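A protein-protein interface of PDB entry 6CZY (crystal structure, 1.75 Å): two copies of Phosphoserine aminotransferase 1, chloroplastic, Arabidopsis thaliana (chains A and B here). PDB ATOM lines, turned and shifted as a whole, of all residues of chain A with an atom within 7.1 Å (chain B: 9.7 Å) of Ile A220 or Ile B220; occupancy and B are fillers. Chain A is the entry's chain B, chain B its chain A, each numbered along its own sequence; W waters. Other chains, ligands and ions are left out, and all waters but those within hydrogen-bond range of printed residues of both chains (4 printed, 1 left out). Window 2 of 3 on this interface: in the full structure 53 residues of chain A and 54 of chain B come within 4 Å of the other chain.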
ATOM      1  N   ALA A  82     -14.487  19.749  19.806  1.00  0.00           N
ATOM      2  CA  ALA A  82     -13.163  19.161  19.746  1.00  0.00           C
ATOM      3  C   ALA A  82     -12.702  18.643  21.089  1.00  0.00           C
ATOM      4  O   ALA A  82     -12.172  17.525  21.191  1.00  0.00           O
ATOM      5  CB  ALA A  82     -12.159  20.172  19.176  1.00  0.00           C
ATOM      6  N   LEU A  86     -11.187  14.767  22.325  1.00  0.00           N
ATOM      7  CA  LEU A  86      -9.754  14.911  22.685  1.00  0.00           C
ATOM      8  C   LEU A  86      -9.527  14.467  24.151  1.00  0.00           C
ATOM      9  O   LEU A  86      -8.539  13.794  24.465  1.00  0.00           O
ATOM     10  CB  LEU A  86      -9.244  16.314  22.484  1.00  0.00           C
ATOM     11  CG  LEU A  86      -8.892  16.741  21.050  1.00  0.00           C
ATOM     12  CD1 LEU A  86      -8.655  18.222  20.983  1.00  0.00           C
ATOM     13  CD2 LEU A  86      -7.671  16.000  20.545  1.00  0.00           C
ATOM     14  N   SER A  91      -7.594   7.884  19.917  1.00  0.00           N
ATOM     15  CA  SER A  91      -7.816   8.159  18.503  1.00  0.00           C
ATOM     16  C   SER A  91      -8.604   7.040  17.802  1.00  0.00           C
ATOM     17  O   SER A  91      -9.276   7.292  16.792  1.00  0.00           O
ATOM     18  CB  SER A  91      -6.457   8.446  17.810  1.00  0.00           C
ATOM     19  OG  SER A  91      -5.632   7.318  17.924  1.00  0.00           O
ATOM     20  N   GLU A 110     -16.699  17.548  13.578  1.00  0.00           N
ATOM     21  CA  GLU A 110     -15.506  17.884  14.366  1.00  0.00           C
ATOM     22  C   GLU A 110     -14.916  16.643  15.058  1.00  0.00           C
ATOM     23  O   GLU A 110     -13.703  16.460  15.047  1.00  0.00           O
ATOM     24  CB  GLU A 110     -15.808  19.005  15.383  1.00  0.00           C
ATOM     25  CG  GLU A 110     -14.597  19.542  16.122  1.00  0.00           C
ATOM     26  CD  GLU A 110     -13.647  20.415  15.293  1.00  0.00           C
ATOM     27  OE1 GLU A 110     -13.704  20.447  14.010  1.00  0.00           O
ATOM     28  OE2 GLU A 110     -12.820  21.103  15.937  1.00  0.00           O
ATOM     29  N   LYS A 113     -12.234  14.186  13.460  1.00  0.00           N
ATOM     30  CA  LYS A 113     -10.813  14.497  13.486  1.00  0.00           C
ATOM     31  C   LYS A 113     -10.024  13.730  14.536  1.00  0.00           C
ATOM     32  O   LYS A 113      -8.786  13.575  14.424  1.00  0.00           O
ATOM     33  CB  LYS A 113     -10.589  15.991  13.751  1.00  0.00           C
ATOM     34  CG  LYS A 113     -10.941  16.928  12.600  1.00  0.00           C
ATOM     35  CD  LYS A 113     -10.805  18.374  13.132  1.00  0.00           C
ATOM     36  CE  LYS A 113     -11.248  19.359  12.115  1.00  0.00           C
ATOM     37  NZ  LYS A 113     -11.220  20.723  12.649  1.00  0.00           N
ATOM     38  N   TYR A 114     -10.712  13.309  15.581  1.00  0.00           N
ATOM     39  CA  TYR A 114     -10.041  12.880  16.823  1.00  0.00           C
ATOM     40  C   TYR A 114     -10.347  11.463  17.249  1.00  0.00           C
ATOM     41  O   TYR A 114      -9.716  10.943  18.189  1.00  0.00           O
ATOM     42  CB  TYR A 114     -10.467  13.827  17.929  1.00  0.00           C
ATOM     43  CG  TYR A 114     -10.126  15.257  17.581  1.00  0.00           C
ATOM     44  CD1 TYR A 114      -8.831  15.626  17.299  1.00  0.00           C
ATOM     45  CD2 TYR A 114     -11.122  16.228  17.439  1.00  0.00           C
ATOM     46  CE1 TYR A 114      -8.524  16.943  16.931  1.00  0.00           C
ATOM     47  CE2 TYR A 114     -10.818  17.510  17.055  1.00  0.00           C
ATOM     48  CZ  TYR A 114      -9.514  17.868  16.830  1.00  0.00           C
ATOM     49  OH  TYR A 114      -9.215  19.159  16.402  1.00  0.00           O
ATOM     50  N   ALA A 217      -6.272  13.026  28.574  1.00  0.00           N
ATOM     51  CA  ALA A 217      -6.538  13.560  27.250  1.00  0.00           C
ATOM     52  C   ALA A 217      -5.477  13.071  26.273  1.00  0.00           C
ATOM     53  O   ALA A 217      -4.392  12.697  26.680  1.00  0.00           O
ATOM     54  CB  ALA A 217      -6.563  15.075  27.242  1.00  0.00           C
ATOM     55  N   GLN A 218      -5.827  13.093  24.993  1.00  0.00           N
ATOM     56  CA  GLN A 218      -4.882  12.805  23.921  1.00  0.00           C
ATOM     57  C   GLN A 218      -3.688  13.776  24.003  1.00  0.00           C
ATOM     58  O   GLN A 218      -3.822  14.961  24.387  1.00  0.00           O
ATOM     59  CB  GLN A 218      -5.569  12.889  22.535  1.00  0.00           C
ATOM     60  CG  GLN A 218      -6.641  11.834  22.325  1.00  0.00           C
ATOM     61  CD  GLN A 218      -7.158  11.763  20.908  1.00  0.00           C
ATOM     62  OE1 GLN A 218      -6.373  11.757  19.960  1.00  0.00           O
ATOM     63  NE2 GLN A 218      -8.452  11.672  20.754  1.00  0.00           N
ATOM     64  N   ASP A 219      -2.497  13.292  23.645  1.00  0.00           N
ATOM     65  CA  ASP A 219      -1.300  14.150  23.698  1.00  0.00           C
ATOM     66  C   ASP A 219      -1.387  15.457  22.902  1.00  0.00           C
ATOM     67  O   ASP A 219      -0.779  16.446  23.295  1.00  0.00           O
ATOM     68  CB  ASP A 219      -0.055  13.383  23.180  1.00  0.00           C
ATOM     69  CG  ASP A 219       0.426  12.315  24.128  1.00  0.00           C
ATOM     70  OD1 ASP A 219      -0.107  12.145  25.270  1.00  0.00           O
ATOM     71  OD2 ASP A 219       1.380  11.598  23.722  1.00  0.00           O
ATOM     72  N   ILE A 220      -2.133  15.448  21.807  1.00  0.00           N
ATOM     73  CA  ILE A 220      -2.292  16.642  20.948  1.00  0.00           C
ATOM     74  C   ILE A 220      -3.310  17.651  21.497  1.00  0.00           C
ATOM     75  O   ILE A 220      -3.557  18.673  20.871  1.00  0.00           O
ATOM     76  CB  ILE A 220      -2.734  16.298  19.518  1.00  0.00           C
ATOM     77  CG1 ILE A 220      -4.001  15.448  19.559  1.00  0.00           C
ATOM     78  CG2 ILE A 220      -1.638  15.562  18.781  1.00  0.00           C
ATOM     79  CD1 ILE A 220      -4.701  15.267  18.228  1.00  0.00           C
ATOM     80  N   THR A 221      -3.924  17.344  22.629  1.00  0.00           N
ATOM     81  CA  THR A 221      -4.916  18.256  23.203  1.00  0.00           C
ATOM     82  C   THR A 221      -4.239  19.595  23.585  1.00  0.00           C
ATOM     83  O   THR A 221      -3.329  19.606  24.388  1.00  0.00           O
ATOM     84  CB  THR A 221      -5.623  17.622  24.395  1.00  0.00           C
ATOM     85  OG1 THR A 221      -6.210  16.343  24.014  1.00  0.00           O
ATOM     86  CG2 THR A 221      -6.737  18.566  24.938  1.00  0.00           C
ATOM     87  N   PRO A 222      -4.715  20.724  23.034  1.00  0.00           N
ATOM     88  CA  PRO A 222      -4.204  22.013  23.516  1.00  0.00           C
ATOM     89  C   PRO A 222      -4.388  22.158  25.026  1.00  0.00           C
ATOM     90  O   PRO A 222      -5.369  21.675  25.545  1.00  0.00           O
ATOM     91  CB  PRO A 222      -5.056  23.030  22.759  1.00  0.00           C
ATOM     92  CG  PRO A 222      -5.480  22.366  21.523  1.00  0.00           C
ATOM     93  CD  PRO A 222      -5.681  20.913  21.923  1.00  0.00           C
ATOM     94  N   VAL A 223      -3.470  22.837  25.749  1.00  0.00           N
ATOM     95  CA  VAL A 223      -3.654  22.953  27.207  1.00  0.00           C
ATOM     96  C   VAL A 223      -5.006  23.615  27.505  1.00  0.00           C
ATOM     97  O   VAL A 223      -5.688  23.290  28.462  1.00  0.00           O
ATOM     98  CB  VAL A 223      -2.442  23.672  27.865  1.00  0.00           C
ATOM     99  CG1 VAL A 223      -2.317  25.126  27.474  1.00  0.00           C
ATOM    100  CG2 VAL A 223      -2.460  23.516  29.387  1.00  0.00           C
ATOM    101  N   ALA B  82      -1.077  27.220  21.095  1.00  0.00           N
ATOM    102  CA  ALA B  82      -1.374  26.046  20.272  1.00  0.00           C
ATOM    103  C   ALA B  82      -1.725  26.391  18.802  1.00  0.00           C
ATOM    104  O   ALA B  82      -1.216  25.779  17.847  1.00  0.00           O
ATOM    105  CB  ALA B  82      -2.499  25.249  20.885  1.00  0.00           C
ATOM    106  N   ALA B  83      -2.561  27.405  18.612  1.00  0.00           N
ATOM    107  CA  ALA B  83      -3.035  27.737  17.254  1.00  0.00           C
ATOM    108  C   ALA B  83      -1.903  28.140  16.295  1.00  0.00           C
ATOM    109  O   ALA B  83      -1.960  27.849  15.086  1.00  0.00           O
ATOM    110  CB  ALA B  83      -4.058  28.860  17.325  1.00  0.00           C
ATOM    111  N   PRO B  85       1.545  27.192  15.977  1.00  0.00           N
ATOM    112  CA  PRO B  85       2.178  26.073  15.246  1.00  0.00           C
ATOM    113  C   PRO B  85       1.162  25.179  14.518  1.00  0.00           C
ATOM    114  O   PRO B  85       1.512  24.621  13.474  1.00  0.00           O
ATOM    115  CB  PRO B  85       2.953  25.330  16.332  1.00  0.00           C
ATOM    116  CG  PRO B  85       2.163  25.651  17.580  1.00  0.00           C
ATOM    117  CD  PRO B  85       1.813  27.100  17.419  1.00  0.00           C
ATOM    118  N   LEU B  86      -0.068  25.049  15.027  1.00  0.00           N
ATOM    119  CA  LEU B  86      -1.073  24.227  14.293  1.00  0.00           C
ATOM    120  C   LEU B  86      -1.343  24.822  12.910  1.00  0.00           C
ATOM    121  O   LEU B  86      -1.435  24.111  11.911  1.00  0.00           O
ATOM    122  CB  LEU B  86      -2.353  24.076  15.102  1.00  0.00           C
ATOM    123  CG  LEU B  86      -2.307  23.000  16.204  1.00  0.00           C
ATOM    124  CD1 LEU B  86      -3.496  23.169  17.167  1.00  0.00           C
ATOM    125  CD2 LEU B  86      -2.312  21.591  15.603  1.00  0.00           C
ATOM    126  N   ASN B  87      -1.447  26.149  12.849  1.00  0.00           N
ATOM    127  CA  ASN B  87      -1.767  26.777  11.579  1.00  0.00           C
ATOM    128  C   ASN B  87      -0.550  26.938  10.659  1.00  0.00           C
ATOM    129  O   ASN B  87      -0.716  26.937   9.433  1.00  0.00           O
ATOM    130  CB  ASN B  87      -2.378  28.144  11.802  1.00  0.00           C
ATOM    131  CG  ASN B  87      -3.833  28.080  12.159  1.00  0.00           C
ATOM    132  OD1 ASN B  87      -4.692  28.132  11.265  1.00  0.00           O
ATOM    133  ND2 ASN B  87      -4.142  27.998  13.463  1.00  0.00           N
ATOM    134  N   CYS B  89       2.727  25.553  10.845  1.00  0.00           N
ATOM    135  CA  CYS B  89       3.761  24.531  10.722  1.00  0.00           C
ATOM    136  C   CYS B  89       3.192  23.202  10.374  1.00  0.00           C
ATOM    137  O   CYS B  89       2.052  22.929  10.687  1.00  0.00           O
ATOM    138  CB  CYS B  89       4.480  24.363  12.038  1.00  0.00           C
ATOM    139  SG  CYS B  89       5.424  25.807  12.546  1.00  0.00           S
ATOM    140  N   LYS B  90       4.007  22.374   9.709  1.00  0.00           N
ATOM    141  CA  LYS B  90       3.784  20.943   9.689  1.00  0.00           C
ATOM    142  C   LYS B  90       4.410  20.330  10.932  1.00  0.00           C
ATOM    143  O   LYS B  90       5.275  20.942  11.565  1.00  0.00           O
ATOM    144  CB  LYS B  90       4.446  20.331   8.422  1.00  0.00           C
ATOM    145  CG  LYS B  90       3.835  20.880   7.144  1.00  0.00           C
ATOM    146  CD  LYS B  90       4.279  20.117   5.904  1.00  0.00           C
ATOM    147  CE  LYS B  90       5.685  20.504   5.505  1.00  0.00           C
ATOM    148  NZ  LYS B  90       5.870  20.373   4.012  1.00  0.00           N
ATOM    149  N   SER B  91       4.065  19.084  11.243  1.00  0.00           N
ATOM    150  CA  SER B  91       4.571  18.473  12.466  1.00  0.00           C
ATOM    151  C   SER B  91       6.093  18.307  12.543  1.00  0.00           C
ATOM    152  O   SER B  91       6.628  18.219  13.626  1.00  0.00           O
ATOM    153  CB  SER B  91       3.881  17.128  12.752  1.00  0.00           C
ATOM    154  OG  SER B  91       4.136  16.257  11.710  1.00  0.00           O
ATOM    155  N   GLU B 110       4.085  24.513  24.865  1.00  0.00           N
ATOM    156  CA  GLU B 110       2.855  24.170  24.140  1.00  0.00           C
ATOM    157  C   GLU B 110       3.164  23.852  22.651  1.00  0.00           C
ATOM    158  O   GLU B 110       2.623  22.863  22.078  1.00  0.00           O
ATOM    159  CB  GLU B 110       1.849  25.332  24.293  1.00  0.00           C
ATOM    160  CG  GLU B 110       0.483  25.080  23.672  1.00  0.00           C
ATOM    161  CD  GLU B 110      -0.372  24.035  24.364  1.00  0.00           C
ATOM    162  OE1 GLU B 110       0.070  23.272  25.275  1.00  0.00           O
ATOM    163  OE2 GLU B 110      -1.567  24.040  24.042  1.00  0.00           O
ATOM    164  N   ALA B 111       4.092  24.614  22.036  1.00  0.00           N
ATOM    165  CA  ALA B 111       4.411  24.394  20.625  1.00  0.00           C
ATOM    166  C   ALA B 111       5.000  22.997  20.392  1.00  0.00           C
ATOM    167  O   ALA B 111       4.784  22.405  19.326  1.00  0.00           O
ATOM    168  CB  ALA B 111       5.397  25.455  20.103  1.00  0.00           C
ATOM    169  N   LYS B 112       5.686  22.453  21.393  1.00  0.00           N
ATOM    170  CA  LYS B 112       6.301  21.122  21.233  1.00  0.00           C
ATOM    171  C   LYS B 112       5.288  20.015  20.934  1.00  0.00           C
ATOM    172  O   LYS B 112       5.639  18.975  20.338  1.00  0.00           O
ATOM    173  CB  LYS B 112       7.114  20.711  22.482  1.00  0.00           C
ATOM    174  CG  LYS B 112       8.414  21.444  22.658  1.00  0.00           C
ATOM    175  CD  LYS B 112       9.191  20.860  23.844  1.00  0.00           C
ATOM    176  CE  LYS B 112      10.561  21.505  23.949  1.00  0.00           C
ATOM    177  NZ  LYS B 112      11.507  21.007  22.891  1.00  0.00           N
ATOM    178  N   LYS B 113       4.034  20.211  21.316  1.00  0.00           N
ATOM    179  CA  LYS B 113       3.004  19.215  20.980  1.00  0.00           C
ATOM    180  C   LYS B 113       2.764  19.119  19.449  1.00  0.00           C
ATOM    181  O   LYS B 113       2.239  18.112  18.953  1.00  0.00           O
ATOM    182  CB  LYS B 113       1.669  19.614  21.599  1.00  0.00           C
ATOM    183  CG  LYS B 113       1.622  19.531  23.103  1.00  0.00           C
ATOM    184  CD  LYS B 113       0.299  20.148  23.565  1.00  0.00           C
ATOM    185  CE  LYS B 113       0.194  20.033  25.059  1.00  0.00           C
ATOM    186  NZ  LYS B 113      -1.000  20.732  25.620  1.00  0.00           N
ATOM    187  N   TYR B 114       3.119  20.171  18.725  1.00  0.00           N
ATOM    188  CA  TYR B 114       2.660  20.368  17.348  1.00  0.00           C
ATOM    189  C   TYR B 114       3.780  20.455  16.291  1.00  0.00           C
ATOM    190  O   TYR B 114       3.488  20.343  15.091  1.00  0.00           O
ATOM    191  CB  TYR B 114       1.748  21.592  17.272  1.00  0.00           C
ATOM    192  CG  TYR B 114       0.633  21.492  18.274  1.00  0.00           C
ATOM    193  CD1 TYR B 114      -0.274  20.451  18.208  1.00  0.00           C
ATOM    194  CD2 TYR B 114       0.505  22.402  19.312  1.00  0.00           C
ATOM    195  CE1 TYR B 114      -1.303  20.333  19.129  1.00  0.00           C
ATOM    196  CE2 TYR B 114      -0.490  22.275  20.261  1.00  0.00           C
ATOM    197  CZ  TYR B 114      -1.413  21.249  20.139  1.00  0.00           C
ATOM    198  OH  TYR B 114      -2.371  21.125  21.093  1.00  0.00           O
ATOM    199  N   CYS B 115       5.020  20.684  16.729  1.00  0.00           N
ATOM    200  CA  CYS B 115       6.179  20.794  15.844  1.00  0.00           C
ATOM    201  C   CYS B 115       7.444  20.755  16.684  1.00  0.00           C
ATOM    202  O   CYS B 115       7.376  20.475  17.897  1.00  0.00           O
ATOM    203  CB  CYS B 115       6.163  22.073  14.995  1.00  0.00           C
ATOM    204  SG  CYS B 115       6.261  23.590  15.922  1.00  0.00           S
ATOM    205  N   ASN B 216      -4.049  26.122   5.136  1.00  0.00           N
ATOM    206  CA  ASN B 216      -3.089  25.034   5.351  1.00  0.00           C
ATOM    207  C   ASN B 216      -2.739  24.675   6.824  1.00  0.00           C
ATOM    208  O   ASN B 216      -1.606  24.273   7.091  1.00  0.00           O
ATOM    209  CB  ASN B 216      -1.771  25.407   4.663  1.00  0.00           C
ATOM    210  CG  ASN B 216      -1.603  24.719   3.360  1.00  0.00           C
ATOM    211  OD1 ASN B 216      -2.222  25.116   2.364  1.00  0.00           O
ATOM    212  ND2 ASN B 216      -0.756  23.677   3.336  1.00  0.00           N
ATOM    213  N   ALA B 217      -3.668  24.832   7.766  1.00  0.00           N
ATOM    214  CA  ALA B 217      -3.485  24.284   9.105  1.00  0.00           C
ATOM    215  C   ALA B 217      -3.319  22.749   9.104  1.00  0.00           C
ATOM    216  O   ALA B 217      -3.750  22.052   8.170  1.00  0.00           O
ATOM    217  CB  ALA B 217      -4.653  24.656   9.981  1.00  0.00           C
ATOM    218  N   GLN B 218      -2.642  22.225  10.117  1.00  0.00           N
ATOM    219  CA  GLN B 218      -2.590  20.768  10.308  1.00  0.00           C
ATOM    220  C   GLN B 218      -3.993  20.153  10.406  1.00  0.00           C
ATOM    221  O   GLN B 218      -4.934  20.763  10.939  1.00  0.00           O
ATOM    222  CB  GLN B 218      -1.780  20.437  11.576  1.00  0.00           C
ATOM    223  CG  GLN B 218      -0.344  20.936  11.516  1.00  0.00           C
ATOM    224  CD  GLN B 218       0.490  20.454  12.672  1.00  0.00           C
ATOM    225  OE1 GLN B 218       0.347  19.294  13.111  1.00  0.00           O
ATOM    226  NE2 GLN B 218       1.397  21.291  13.132  1.00  0.00           N
ATOM    227  N   ASP B 219      -4.143  18.918   9.904  1.00  0.00           N
ATOM    228  CA  ASP B 219      -5.464  18.248   9.936  1.00  0.00           C
ATOM    229  C   ASP B 219      -6.090  18.131  11.311  1.00  0.00           C
ATOM    230  O   ASP B 219      -7.304  18.224  11.449  1.00  0.00           O
ATOM    231  CB  ASP B 219      -5.383  16.843   9.326  1.00  0.00           C
ATOM    232  CG  ASP B 219      -5.051  16.857   7.846  1.00  0.00           C
ATOM    233  OD1 ASP B 219      -5.183  17.909   7.170  1.00  0.00           O
ATOM    234  OD2 ASP B 219      -4.646  15.766   7.324  1.00  0.00           O
ATOM    235  N   ILE B 220      -5.280  17.994  12.344  1.00  0.00           N
ATOM    236  CA  ILE B 220      -5.800  17.910  13.723  1.00  0.00           C
ATOM    237  C   ILE B 220      -6.233  19.257  14.383  1.00  0.00           C
ATOM    238  O   ILE B 220      -6.650  19.274  15.555  1.00  0.00           O
ATOM    239  CB  ILE B 220      -4.754  17.262  14.673  1.00  0.00           C
ATOM    240  CG1 ILE B 220      -3.414  18.025  14.572  1.00  0.00           C
ATOM    241  CG2 ILE B 220      -4.679  15.763  14.393  1.00  0.00           C
ATOM    242  CD1 ILE B 220      -2.492  17.847  15.772  1.00  0.00           C
ATOM    243  N   THR B 221      -6.068  20.364  13.672  1.00  0.00           N
ATOM    244  CA  THR B 221      -6.458  21.680  14.220  1.00  0.00           C
ATOM    245  C   THR B 221      -7.950  21.718  14.498  1.00  0.00           C
ATOM    246  O   THR B 221      -8.755  21.498  13.580  1.00  0.00           O
ATOM    247  CB  THR B 221      -6.057  22.792  13.224  1.00  0.00           C
ATOM    248  OG1 THR B 221      -4.668  22.655  12.906  1.00  0.00           O
ATOM    249  CG2 THR B 221      -6.351  24.173  13.801  1.00  0.00           C
ATOM    250  N   PRO B 222      -8.346  22.025  15.735  1.00  0.00           N
ATOM    251  CA  PRO B 222      -9.773  22.253  15.961  1.00  0.00           C
ATOM    252  C   PRO B 222     -10.282  23.344  15.057  1.00  0.00           C
ATOM    253  O   PRO B 222      -9.543  24.325  14.787  1.00  0.00           O
ATOM    254  CB  PRO B 222      -9.850  22.722  17.416  1.00  0.00           C
ATOM    255  CG  PRO B 222      -8.627  22.136  18.033  1.00  0.00           C
ATOM    256  CD  PRO B 222      -7.567  22.152  16.984  1.00  0.00           C
ATOM    257  N   VAL B 223     -11.542  23.236  14.652  1.00  0.00           N
ATOM    258  CA  VAL B 223     -12.118  24.301  13.797  1.00  0.00           C
ATOM    259  C   VAL B 223     -12.011  25.666  14.470  1.00  0.00           C
ATOM    260  O   VAL B 223     -11.750  26.666  13.811  1.00  0.00           O
ATOM    261  CB  VAL B 223     -13.556  23.963  13.340  1.00  0.00           C
ATOM    262  CG1 VAL B 223     -14.601  24.098  14.433  1.00  0.00           C
ATOM    263  CG2 VAL B 223     -13.957  24.821  12.144  1.00  0.00           C
ATOM    264  N   MET B 224     -12.134  25.700  15.798  1.00  0.00           N
ATOM    265  CA  MET B 224     -12.060  26.969  16.520  1.00  0.00           C
ATOM    266  C   MET B 224     -10.673  27.546  16.648  1.00  0.00           C
ATOM    267  O   MET B 224     -10.531  28.670  17.114  1.00  0.00           O
ATOM    268  CB  MET B 224     -12.661  26.830  17.920  1.00  0.00           C
ATOM    269  CG  MET B 224     -14.163  26.758  17.864  1.00  0.00           C
ATOM    270  SD  MET B 224     -14.982  28.180  17.074  1.00  0.00           S
ATOM    271  CE  MET B 224     -14.375  29.495  18.117  1.00  0.00           C
ATOM    272  N   LEU B 225      -9.659  26.785  16.296  1.00  0.00           N
ATOM    273  CA  LEU B 225      -8.307  27.330  16.268  1.00  0.00           C
ATOM    274  C   LEU B 225      -7.796  27.633  14.859  1.00  0.00           C
ATOM    275  O   LEU B 225      -6.636  28.040  14.731  1.00  0.00           O
ATOM    276  CB  LEU B 225      -7.333  26.379  16.972  1.00  0.00           C
ATOM    277  CG  LEU B 225      -7.224  26.544  18.495  1.00  0.00           C
ATOM    278  CD1 LEU B 225      -8.506  26.307  19.269  1.00  0.00           C
ATOM    279  CD2 LEU B 225      -6.119  25.683  19.019  1.00  0.00           C
ATOM    280  N   ASP B 226      -8.643  27.443  13.831  1.00  0.00           N
ATOM    281  CA  ASP B 226      -8.206  27.494  12.427  1.00  0.00           C
ATOM    282  C   ASP B 226      -8.302  28.926  11.886  1.00  0.00           C
ATOM    283  O   ASP B 226      -9.417  29.487  11.835  1.00  0.00           O
ATOM    284  CB  ASP B 226      -9.091  26.558  11.622  1.00  0.00           C
ATOM    285  CG  ASP B 226      -8.639  26.422  10.164  1.00  0.00           C
ATOM    286  OD1 ASP B 226      -8.695  27.393   9.433  1.00  0.00           O
ATOM    287  OD2 ASP B 226      -8.252  25.339   9.755  1.00  0.00           O
HETATM  288  O   HOH W   1      -3.610  25.964  24.317  1.00  0.00           O
HETATM  289  O   HOH W   2      -9.385  23.015  11.158  1.00  0.00           O
HETATM  290  O   HOH W   3     -13.340  23.332  17.621  1.00  0.00           O
HETATM  291  O   HOH W   4      -8.441  20.838  10.688  1.00  0.00           O
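OE2 of Glu B110 is in hydrogen-bond range of N of Val A223 (2.8 Å). The backbone carbonyl oxygen (O) of Thr B221 is in hydrogen-bond range of the side-chain amino group (NZ) of Lys A113, at 2.7 Å. The backbone NH (N) of Val A223 sits close to the side-chain amino group (NZ) of Lys B113 (3.2 Å). The backbone carbonyl oxygen of Ile B220 is in hydrogen-bond range of the side-chain hydroxyl of Tyr A114 (2.7 Å). NZ of Lys A113 sits close to N of Val B223, 3.2 Å away. The side-chain hydroxyl (OH) of Tyr A114 sits close to the backbone nitrogen (N) of Pro B222, at 3.1 Å. OE2 of Glu A110 is in hydrogen-bond range of N of Val B223 (2.8 Å). The backbone carbonyl oxygen (O) of Ile A220 is in hydrogen-bond range of the side-chain hydroxyl (OH) of Tyr B114, at 2.7 Å. N of Pro A222 sits close to OH of Tyr B114. The side-chain amino group (NZ) of Lys B113 sits at hydrogen-bond distance from the backbone carbonyl oxygen (O) of Thr A221.
The backbone carbonyl oxygen (O) of Gln A218 sits at hydrogen-bond distance from the side-chain hydroxyl (OG1) of Thr A221 (2.8 Å). The side-chain carboxylate (OE1) of Glu A110 is in salt-bridge range of the side-chain amino group (NZ) of Lys A113, at 2.8 Å. The backbone carbonyl oxygen (O) of Tyr A114 lies within hydrogen-bond range of the side-chain amide nitrogen (NE2) of Gln A218 (3.0 Å). OE1 of Glu B110 is in salt-bridge range of NZ of Lys B113, 2.8 Å away. O of Tyr B114 sits at hydrogen-bond distance from NE2 of Gln B218, 3.0 Å away. The backbone carbonyl oxygen (O) of Leu A86 sits close to the side-chain hydroxyl (OG1) of Thr A221, at 3.5 Å.
Pro B222 touches Ala A82 (CB to CB, 3.9 Å). Glu A110 touches Pro B222. Lys A113 touches Asp B219. Lys A113 touches Pro B222 (NZ to C, 3.7 Å). C of Thr B221 touches OH of Tyr A114 (3.4 Å). CD of Lys B113 touches O of Asp A219, at 3.9 Å. CD1 of Ile A220 touches CG2 of Ile B220, 3.9 Å away. Pro A222 touches Ala B82 (CB to CB, 3.9 Å). Glu B110 touches Pro A222 (OE2 to CA, 3.4 Å). Lys B113 touches Pro A222.
Of chain B, only Tyr B114 and Ile B220 come within 4 Å of Ile A220. Ile B220 touches just these residues of chain A: Tyr A114 (2.7 Å) and Ile A220 (3.9 Å). Asp A219 touches just one residue of chain B: Lys B113 (3.9 Å). Thr A221 touches two residues of chain B. Of the printed residues of chain A, Asp B219 touches Lys A113 (3.9 Å). Of the printed residues of chain B, Pro A222 touches Ala B82, Glu B110, Lys B113 and Tyr B114. Met B224 touches none of the printed residues of chain A. The nearest residue of chain B that does not touch Ile A220 is Lys B113 (4.6 Å). The nearest residue of chain A that does not touch Ile B220 is Lys A113 (4.7 Å).
Hydrophobic or aromatic side chains of chain B within 4 Å of the printed part of chain A: Ala B82, Tyr B114, Ile B220, Pro B222 and Val B223. Printed residues of chain A that touch a printed residue of chain B: Ala A82, Glu A110, Lys A113, Tyr A114, Asp A219, Ile A220, Thr A221, Pro A222 and Val A223. Hydrophobic or aromatic side chains of chain A within 4 Å of the printed part of chain B: Ala A82, Tyr A114, Ile A220, Pro A222 and Val A223. Among the printed residues, no Asp or Glu carboxylate lies within 4 Å of a Lys or Arg side-chain nitrogen of the other chain.
Glu A110 touches Val B223, and with the chains exchanged Val A223 touches Glu B110. Lys A113 touches Val B223, and with the chains exchanged Val A223 touches Lys B113. Tyr A114 touches Ile B220, and with the chains exchanged Ile A220 touches Tyr B114. Ile A220 touches its own counterpart, Ile B220. 13 positions are printed for both chains. Of the 21 pairs that touch across the chains among the printed residues, 21 have their exchanged pair printed and touching as well.
Water W1 bridges the side-chain carboxylate (OE2) of Glu B110 and the backbone NH (N) of Val A223. Water W3 lies within hydrogen-bond range of OE2 of Glu A110 (2.8 Å), N of Met B224 (3.2 Å) and N of Val B223 (3.5 Å). Water W2 lies within hydrogen-bond range of the backbone carbonyl oxygen of Thr B221 (2.9 Å), the side-chain carboxylate of Asp B226 (2.9 Å) and the side-chain amino group of Lys A113 (3.3 Å). Water W4 lies within hydrogen-bond range of the backbone carbonyl oxygen of Asp B219 (3.0 Å), the backbone carbonyl oxygen of Thr B221 (3.0 Å) and the side-chain amino group of Lys A113 (3.4 Å).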
